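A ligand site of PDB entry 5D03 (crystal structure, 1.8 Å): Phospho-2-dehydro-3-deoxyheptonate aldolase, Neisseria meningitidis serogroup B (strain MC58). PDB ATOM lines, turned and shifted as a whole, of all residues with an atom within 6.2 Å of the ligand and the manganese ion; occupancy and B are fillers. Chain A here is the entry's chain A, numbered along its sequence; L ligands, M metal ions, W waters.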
ATOM      1  N   CYS A  63      30.151 -26.868  16.076  1.00  0.00           N
ATOM      2  CA  CYS A  63      29.244 -26.522  17.137  1.00  0.00           C
ATOM      3  C   CYS A  63      28.397 -27.736  17.487  1.00  0.00           C
ATOM      4  O   CYS A  63      28.208 -28.099  18.661  1.00  0.00           O
ATOM      5  CB  CYS A  63      28.362 -25.344  16.681  1.00  0.00           C
ATOM      6  SG  CYS A  63      26.993 -24.974  17.860  1.00  0.00           S
ATOM      7  N   SER A  64      27.872 -28.394  16.468  1.00  0.00           N
ATOM      8  CA  SER A  64      27.147 -29.615  16.640  1.00  0.00           C
ATOM      9  C   SER A  64      27.460 -30.635  15.548  1.00  0.00           C
ATOM     10  O   SER A  64      27.796 -30.275  14.403  1.00  0.00           O
ATOM     11  CB  SER A  64      25.645 -29.324  16.593  1.00  0.00           C
ATOM     12  OG  SER A  64      25.237 -28.773  15.329  1.00  0.00           O
ATOM     13  N   ARG A  94      35.711 -31.536  19.112  1.00  0.00           N
ATOM     14  CA  ARG A  94      34.350 -31.263  19.570  1.00  0.00           C
ATOM     15  C   ARG A  94      33.455 -32.242  18.870  1.00  0.00           C
ATOM     16  O   ARG A  94      33.331 -32.215  17.643  1.00  0.00           O
ATOM     17  CB  ARG A  94      33.858 -29.843  19.222  1.00  0.00           C
ATOM     18  CG  ARG A  94      34.330 -28.754  20.127  1.00  0.00           C
ATOM     19  CD  ARG A  94      33.757 -27.371  19.794  1.00  0.00           C
ATOM     20  NE  ARG A  94      32.306 -27.364  19.761  1.00  0.00           N
ATOM     21  CZ  ARG A  94      31.510 -26.717  20.609  1.00  0.00           C
ATOM     22  NH1 ARG A  94      31.983 -25.982  21.613  1.00  0.00           N
ATOM     23  NH2 ARG A  94      30.223 -26.835  20.462  1.00  0.00           N
ATOM     24  N   TYR A  96      29.803 -32.778  19.664  1.00  0.00           N
ATOM     25  CA  TYR A  96      28.635 -32.410  20.481  1.00  0.00           C
ATOM     26  C   TYR A  96      27.329 -32.957  19.960  1.00  0.00           C
ATOM     27  O   TYR A  96      26.904 -32.677  18.822  1.00  0.00           O
ATOM     28  CB  TYR A  96      28.582 -30.912  20.600  1.00  0.00           C
ATOM     29  CG  TYR A  96      29.525 -30.265  21.615  1.00  0.00           C
ATOM     30  CD1 TYR A  96      30.863 -30.642  21.741  1.00  0.00           C
ATOM     31  CD2 TYR A  96      29.073 -29.305  22.468  1.00  0.00           C
ATOM     32  CE1 TYR A  96      31.717 -30.045  22.666  1.00  0.00           C
ATOM     33  CE2 TYR A  96      29.930 -28.689  23.378  1.00  0.00           C
ATOM     34  CZ  TYR A  96      31.265 -29.058  23.454  1.00  0.00           C
ATOM     35  OH  TYR A  96      32.141 -28.500  24.355  1.00  0.00           O
ATOM     36  N   GLU A  98      24.363 -33.060  21.917  1.00  0.00           N
ATOM     37  CA  GLU A  98      23.222 -32.418  22.649  1.00  0.00           C
ATOM     38  C   GLU A  98      23.419 -30.898  22.738  1.00  0.00           C
ATOM     39  O   GLU A  98      24.421 -30.418  23.285  1.00  0.00           O
ATOM     40  CB  GLU A  98      23.122 -33.001  24.068  1.00  0.00           C
ATOM     41  CG  GLU A  98      23.189 -34.504  24.039  1.00  0.00           C
ATOM     42  CD  GLU A  98      23.023 -35.152  25.409  1.00  0.00           C
ATOM     43  OE1 GLU A  98      23.576 -34.620  26.430  1.00  0.00           O
ATOM     44  OE2 GLU A  98      22.347 -36.202  25.383  1.00  0.00           O
ATOM     45  N   LYS A  99      22.393 -30.191  22.296  1.00  0.00           N
ATOM     46  CA  LYS A  99      22.420 -28.736  22.213  1.00  0.00           C
ATOM     47  C   LYS A  99      21.332 -28.099  23.042  1.00  0.00           C
ATOM     48  O   LYS A  99      20.134 -28.446  22.901  1.00  0.00           O
ATOM     49  CB  LYS A  99      22.216 -28.327  20.746  1.00  0.00           C
ATOM     50  CG  LYS A  99      23.197 -28.951  19.777  1.00  0.00           C
ATOM     51  CD  LYS A  99      24.672 -28.686  20.129  1.00  0.00           C
ATOM     52  CE  LYS A  99      25.103 -27.229  20.146  1.00  0.00           C
ATOM     53  NZ  LYS A  99      26.472 -27.019  20.644  1.00  0.00           N
ATOM     54  N   PRO A 100      21.721 -27.112  23.876  1.00  0.00           N
ATOM     55  CA  PRO A 100      20.758 -26.388  24.710  1.00  0.00           C
ATOM     56  C   PRO A 100      20.204 -25.251  23.901  1.00  0.00           C
ATOM     57  O   PRO A 100      20.970 -24.463  23.375  1.00  0.00           O
ATOM     58  CB  PRO A 100      21.604 -25.898  25.881  1.00  0.00           C
ATOM     59  CG  PRO A 100      23.003 -25.795  25.394  1.00  0.00           C
ATOM     60  CD  PRO A 100      23.138 -26.845  24.289  1.00  0.00           C
ATOM     61  N   GLU A 145      29.312 -31.886  25.222  1.00  0.00           N
ATOM     62  CA  GLU A 145      28.592 -31.286  26.318  1.00  0.00           C
ATOM     63  C   GLU A 145      27.630 -32.328  26.839  1.00  0.00           C
ATOM     64  O   GLU A 145      26.837 -32.895  26.064  1.00  0.00           O
ATOM     65  CB  GLU A 145      27.772 -30.006  25.912  1.00  0.00           C
ATOM     66  CG  GLU A 145      26.950 -29.514  27.102  1.00  0.00           C
ATOM     67  CD  GLU A 145      26.020 -28.312  26.871  1.00  0.00           C
ATOM     68  OE1 GLU A 145      26.249 -27.552  25.906  1.00  0.00           O
ATOM     69  OE2 GLU A 145      25.090 -28.141  27.715  1.00  0.00           O
ATOM     70  N   ALA A 163      31.994 -30.994  28.773  1.00  0.00           N
ATOM     71  CA  ALA A 163      31.560 -29.656  29.148  1.00  0.00           C
ATOM     72  C   ALA A 163      30.216 -29.690  29.793  1.00  0.00           C
ATOM     73  O   ALA A 163      29.343 -30.527  29.435  1.00  0.00           O
ATOM     74  CB  ALA A 163      31.502 -28.704  27.949  1.00  0.00           C
ATOM     75  N   ILE A 164      30.047 -28.793  30.751  1.00  0.00           N
ATOM     76  CA  ILE A 164      28.732 -28.398  31.267  1.00  0.00           C
ATOM     77  C   ILE A 164      28.487 -26.964  30.786  1.00  0.00           C
ATOM     78  O   ILE A 164      29.272 -26.032  30.992  1.00  0.00           O
ATOM     79  CB  ILE A 164      28.609 -28.509  32.796  1.00  0.00           C
ATOM     80  CG1 ILE A 164      28.927 -29.933  33.265  1.00  0.00           C
ATOM     81  CG2 ILE A 164      27.211 -28.091  33.275  1.00  0.00           C
ATOM     82  CD1 ILE A 164      27.958 -31.029  32.884  1.00  0.00           C
ATOM     83  N   GLY A 165      27.372 -26.797  30.091  1.00  0.00           N
ATOM     84  CA  GLY A 165      27.107 -25.530  29.404  1.00  0.00           C
ATOM     85  C   GLY A 165      26.767 -24.404  30.326  1.00  0.00           C
ATOM     86  O   GLY A 165      26.382 -24.595  31.479  1.00  0.00           O
ATOM     87  N   ALA A 166      26.863 -23.215  29.775  1.00  0.00           N
ATOM     88  CA  ALA A 166      26.568 -21.993  30.484  1.00  0.00           C
ATOM     89  C   ALA A 166      25.204 -22.053  31.127  1.00  0.00           C
ATOM     90  O   ALA A 166      25.024 -21.523  32.216  1.00  0.00           O
ATOM     91  CB  ALA A 166      26.641 -20.842  29.551  1.00  0.00           C
ATOM     92  N   ARG A 167      24.262 -22.684  30.455  1.00  0.00           N
ATOM     93  CA  ARG A 167      22.848 -22.644  30.894  1.00  0.00           C
ATOM     94  C   ARG A 167      22.564 -23.660  32.029  1.00  0.00           C
ATOM     95  O   ARG A 167      21.471 -23.689  32.546  1.00  0.00           O
ATOM     96  CB  ARG A 167      21.937 -22.909  29.731  1.00  0.00           C
ATOM     97  CG  ARG A 167      22.003 -21.759  28.736  1.00  0.00           C
ATOM     98  CD  ARG A 167      21.271 -22.017  27.431  1.00  0.00           C
ATOM     99  NE  ARG A 167      21.560 -20.929  26.486  1.00  0.00           N
ATOM    100  CZ  ARG A 167      22.697 -20.815  25.782  1.00  0.00           C
ATOM    101  NH1 ARG A 167      23.680 -21.729  25.856  1.00  0.00           N
ATOM    102  NH2 ARG A 167      22.872 -19.782  24.968  1.00  0.00           N
ATOM    103  N   LYS A 188      31.271 -23.896  32.112  1.00  0.00           N
ATOM    104  CA  LYS A 188      31.223 -22.575  31.509  1.00  0.00           C
ATOM    105  C   LYS A 188      30.635 -21.553  32.449  1.00  0.00           C
ATOM    106  O   LYS A 188      29.752 -21.863  33.210  1.00  0.00           O
ATOM    107  CB  LYS A 188      30.409 -22.647  30.272  1.00  0.00           C
ATOM    108  CG  LYS A 188      31.189 -23.375  29.207  1.00  0.00           C
ATOM    109  CD  LYS A 188      30.513 -23.315  27.910  1.00  0.00           C
ATOM    110  CE  LYS A 188      31.567 -23.131  26.845  1.00  0.00           C
ATOM    111  NZ  LYS A 188      30.901 -22.859  25.551  1.00  0.00           N
ATOM    112  N   ASN A 189      31.086 -20.309  32.364  1.00  0.00           N
ATOM    113  CA  ASN A 189      30.490 -19.228  33.145  1.00  0.00           C
ATOM    114  C   ASN A 189      29.089 -18.958  32.600  1.00  0.00           C
ATOM    115  O   ASN A 189      28.774 -19.385  31.508  1.00  0.00           O
ATOM    116  CB  ASN A 189      31.349 -17.963  33.098  1.00  0.00           C
ATOM    117  CG  ASN A 189      31.477 -17.375  31.704  1.00  0.00           C
ATOM    118  OD1 ASN A 189      32.555 -17.419  31.118  1.00  0.00           O
ATOM    119  ND2 ASN A 189      30.412 -16.825  31.182  1.00  0.00           N
ATOM    120  N   THR A 191      25.429 -17.258  31.224  1.00  0.00           N
ATOM    121  CA  THR A 191      25.162 -16.582  29.950  1.00  0.00           C
ATOM    122  C   THR A 191      25.302 -15.076  30.049  1.00  0.00           C
ATOM    123  O   THR A 191      25.591 -14.444  29.070  1.00  0.00           O
ATOM    124  CB  THR A 191      23.774 -16.935  29.356  1.00  0.00           C
ATOM    125  OG1 THR A 191      22.740 -16.788  30.350  1.00  0.00           O
ATOM    126  CG2 THR A 191      23.772 -18.345  28.861  1.00  0.00           C
ATOM    127  N   ARG A 236      33.640 -17.935  28.565  1.00  0.00           N
ATOM    128  CA  ARG A 236      32.939 -17.943  27.264  1.00  0.00           C
ATOM    129  C   ARG A 236      32.150 -16.662  26.965  1.00  0.00           C
ATOM    130  O   ARG A 236      31.250 -16.627  26.094  1.00  0.00           O
ATOM    131  CB  ARG A 236      32.043 -19.210  27.141  1.00  0.00           C
ATOM    132  CG  ARG A 236      31.062 -19.505  28.275  1.00  0.00           C
ATOM    133  CD  ARG A 236      29.839 -18.582  28.297  1.00  0.00           C
ATOM    134  NE  ARG A 236      28.851 -18.891  27.246  1.00  0.00           N
ATOM    135  CZ  ARG A 236      27.864 -18.083  26.853  1.00  0.00           C
ATOM    136  NH1 ARG A 236      27.003 -18.453  25.907  1.00  0.00           N
ATOM    137  NH2 ARG A 236      27.762 -16.882  27.354  1.00  0.00           N
ATOM    138  N   ASP A 267      37.075 -19.993  25.789  1.00  0.00           N
ATOM    139  CA  ASP A 267      36.275 -20.260  24.602  1.00  0.00           C
ATOM    140  C   ASP A 267      36.452 -19.055  23.660  1.00  0.00           C
ATOM    141  O   ASP A 267      36.112 -17.947  24.032  1.00  0.00           O
ATOM    142  CB  ASP A 267      34.792 -20.510  25.006  1.00  0.00           C
ATOM    143  CG  ASP A 267      33.863 -20.883  23.784  1.00  0.00           C
ATOM    144  OD1 ASP A 267      34.336 -20.965  22.625  1.00  0.00           O
ATOM    145  OD2 ASP A 267      32.663 -21.104  24.023  1.00  0.00           O
ATOM    146  N   SER A 269      34.648 -18.701  20.979  1.00  0.00           N
ATOM    147  CA  SER A 269      33.356 -18.524  20.297  1.00  0.00           C
ATOM    148  C   SER A 269      32.298 -17.990  21.274  1.00  0.00           C
ATOM    149  O   SER A 269      32.629 -17.286  22.274  1.00  0.00           O
ATOM    150  CB  SER A 269      32.928 -19.870  19.706  1.00  0.00           C
ATOM    151  OG  SER A 269      32.042 -19.716  18.623  1.00  0.00           O
ATOM    152  N   HIS A 270      31.046 -18.312  20.960  1.00  0.00           N
ATOM    153  CA  HIS A 270      29.875 -17.885  21.726  1.00  0.00           C
ATOM    154  C   HIS A 270      29.959 -16.433  22.100  1.00  0.00           C
ATOM    155  O   HIS A 270      30.146 -15.597  21.221  1.00  0.00           O
ATOM    156  CB  HIS A 270      29.678 -18.853  22.880  1.00  0.00           C
ATOM    157  CG  HIS A 270      29.573 -20.238  22.372  1.00  0.00           C
ATOM    158  ND1 HIS A 270      30.617 -21.142  22.427  1.00  0.00           N
ATOM    159  CD2 HIS A 270      28.576 -20.854  21.669  1.00  0.00           C
ATOM    160  CE1 HIS A 270      30.266 -22.248  21.797  1.00  0.00           C
ATOM    161  NE2 HIS A 270      29.033 -22.103  21.338  1.00  0.00           N
ATOM    162  N   ALA A 271      29.866 -16.098  23.370  1.00  0.00           N
ATOM    163  CA  ALA A 271      29.813 -14.686  23.744  1.00  0.00           C
ATOM    164  C   ALA A 271      31.175 -13.993  23.767  1.00  0.00           C
ATOM    165  O   ALA A 271      31.259 -12.782  23.967  1.00  0.00           O
ATOM    166  CB  ALA A 271      29.110 -14.498  25.068  1.00  0.00           C
ATOM    167  N   MET A 302      38.925 -23.311  23.429  1.00  0.00           N
ATOM    168  CA  MET A 302      37.834 -23.913  22.709  1.00  0.00           C
ATOM    169  C   MET A 302      37.544 -23.110  21.457  1.00  0.00           C
ATOM    170  O   MET A 302      37.552 -21.884  21.487  1.00  0.00           O
ATOM    171  CB  MET A 302      36.583 -24.021  23.607  1.00  0.00           C
ATOM    172  CG  MET A 302      35.367 -24.586  22.917  1.00  0.00           C
ATOM    173  SD  MET A 302      33.869 -24.678  24.043  1.00  0.00           S
ATOM    174  CE  MET A 302      34.553 -25.675  25.353  1.00  0.00           C
ATOM    175  N   GLU A 304      35.064 -23.225  17.628  1.00  0.00           N
ATOM    176  CA  GLU A 304      34.011 -23.728  16.796  1.00  0.00           C
ATOM    177  C   GLU A 304      34.439 -23.682  15.347  1.00  0.00           C
ATOM    178  O   GLU A 304      34.543 -22.626  14.756  1.00  0.00           O
ATOM    179  CB  GLU A 304      32.722 -22.951  17.056  1.00  0.00           C
ATOM    180  CG  GLU A 304      32.087 -23.439  18.362  1.00  0.00           C
ATOM    181  CD  GLU A 304      30.675 -22.941  18.569  1.00  0.00           C
ATOM    182  OE1 GLU A 304      30.378 -21.735  18.392  1.00  0.00           O
ATOM    183  OE2 GLU A 304      29.865 -23.779  18.936  1.00  0.00           O
ATOM    184  N   THR A 323      23.939 -25.174  13.347  1.00  0.00           N
ATOM    185  CA  THR A 323      23.736 -24.432  14.585  1.00  0.00           C
ATOM    186  C   THR A 323      24.620 -23.171  14.506  1.00  0.00           C
ATOM    187  O   THR A 323      24.536 -22.445  13.520  1.00  0.00           O
ATOM    188  CB  THR A 323      23.956 -25.354  15.811  1.00  0.00           C
ATOM    189  OG1 THR A 323      25.167 -26.110  15.713  1.00  0.00           O
ATOM    190  CG2 THR A 323      22.816 -26.343  15.903  1.00  0.00           C
ATOM    191  N   ASP A 324      25.503 -22.928  15.476  1.00  0.00           N
ATOM    192  CA  ASP A 324      26.319 -21.716  15.446  1.00  0.00           C
ATOM    193  C   ASP A 324      27.273 -21.741  14.250  1.00  0.00           C
ATOM    194  O   ASP A 324      27.795 -22.805  13.842  1.00  0.00           O
ATOM    195  CB  ASP A 324      27.157 -21.575  16.734  1.00  0.00           C
ATOM    196  CG  ASP A 324      26.296 -21.398  17.970  1.00  0.00           C
ATOM    197  OD1 ASP A 324      25.192 -20.877  17.864  1.00  0.00           O
ATOM    198  OD2 ASP A 324      26.716 -21.787  19.055  1.00  0.00           O
HETATM  199  C1  LIG L   1      28.684 -24.916  23.049  1.00  0.00           C
HETATM  200  O1  LIG L   1      29.890 -24.910  23.440  1.00  0.00           O
HETATM  201  O2  LIG L   1      28.301 -25.293  21.932  1.00  0.00           O
HETATM  202  C2  LIG L   1      27.674 -24.305  23.891  1.00  0.00           C
HETATM  203  C3  LIG L   1      26.403 -24.708  23.879  1.00  0.00           C
HETATM  204  O3  LIG L   1      28.185 -23.163  24.581  1.00  0.00           O
HETATM  205  P1  LIG L   1      27.488 -22.284  25.807  1.00  0.00           P
HETATM  206  O4  LIG L   1      27.016 -23.288  26.855  1.00  0.00           O
HETATM  207  O5  LIG L   1      28.692 -21.437  26.146  1.00  0.00           O
HETATM  208  O6  LIG L   1      26.379 -21.541  25.128  1.00  0.00           O
HETATM  209 MN    MN M   1      27.929 -23.403  19.697  1.00  0.00          MN
HETATM  210  O   HOH W   1      30.774 -26.251  25.480  1.00  0.00           O
HETATM  211  O   HOH W   2      28.323 -26.066  26.461  1.00  0.00           O
HETATM  212  O   HOH W   3      26.241 -24.066  20.726  1.00  0.00           O
HETATM  213  O   HOH W   4      25.324 -19.794  23.431  1.00  0.00           O
HETATM  214  O   HOH W   5      24.354 -23.785  27.747  1.00  0.00           O
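Within 4 Å of the manganese ion: Cys 63, His 270, Glu 304 and Asp 324.
The manganese ion is bound by water W3 (2.1 Å), the side-chain carboxylate (OE2) of Glu 304 (2.1 Å), the side-chain carboxylate (OD2) of Asp 324 (2.1 Å), a ring nitrogen (NE2) of His 270 (2.4 Å) and the side-chain sulfur (SG) of Cys 63 (2.6 Å). The manganese ion has five donor atoms within binding distance.
A ring nitrogen (NE2) of His 270 lies close to an oxygen (O2) of the ligand (3.3 Å). NZ of Lys 99 is in salt-bridge range of O2 of the ligand, at 2.8 Å. The guanidinium group of Arg 94 lies within salt-bridge range of an oxygen (O2) of the ligand (2.9 Å). The backbone NH (N) of Ala 166 lies within hydrogen-bond range of an oxygen (O4) of the ligand. The guanidinium group (NE) of Arg 236 is in salt-bridge range of an oxygen (O5) of the ligand (2.8 Å). O5 of the ligand is in salt-bridge range of NZ of Lys 188 (2.7 Å). NH1 of Arg 167 is in salt-bridge range of O6 of the ligand, at 2.8 Å.
Water W3 bridges an oxygen (O2) of the ligand (2.7 Å) and the side-chain amino group (NZ) of Lys 99 (3.0 Å). Water W1 lies within hydrogen-bond range of O1 of the ligand (2.6 Å), OH of Tyr 96 (2.9 Å), NZ of Lys 188 (3.4 Å) and SD of Met 302 (3.8 Å). Water W4 lies within hydrogen-bond range of an oxygen (O6) of the ligand (2.7 Å), the guanidinium group (NH2) of Arg 167 (2.9 Å) and the guanidinium group (NH1) of Arg 236 (3.3 Å). Water W5 lies within hydrogen-bond range of O4 of the ligand (2.9 Å), NH1 of Arg 167 (2.9 Å) and N of Ala 166 (3.3 Å). Water W2 lies within hydrogen-bond range of the side-chain carboxylate of Glu 145 and an oxygen (O4) of the ligand.
The backbone NH (N) of Arg 236 sits at hydrogen-bond distance from the side-chain amide oxygen (OD1) of Asn 189, 2.8 Å away. NZ of Lys 99 is in hydrogen-bond range of O of Cys 63 (2.8 Å). OD2 of Asp 267 is in salt-bridge range of NZ of Lys 188, at 2.9 Å. O of Ile 164 is in hydrogen-bond range of N of Lys 188, 3.1 Å away. SD of Met 302 sits at hydrogen-bond distance from NZ of Lys 188 (3.8 Å). The backbone carbonyl oxygen (O) of Cys 63 sits at hydrogen-bond distance from the guanidinium group (NH2) of Arg 94, at 3.0 Å. OG1 of Thr 323 sits close to SG of Cys 63, at 3.0 Å. NH1 of Arg 94 sits at hydrogen-bond distance from SD of Met 302.
Merely in contact with the ligand: Gly 165 (3.4 Å), Glu 145 (3.5 Å), Tyr 96 (3.8 Å) and Pro 100 (3.9 Å). Hydrophobic or aromatic side chains within 4 Å of the ligand: Tyr 96, Pro 100, Ala 166 and His 270. 12 residues have an atom within 4 Å of the ligand: Arg 94, Tyr 96, Lys 99, Pro 100, Glu 145, Gly 165, Ala 166, Arg 167, Lys 188, Arg 236, His 270 and Glu 304. The nearest printed residue that does not touch the ligand is Met 302 (4.03 Å).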
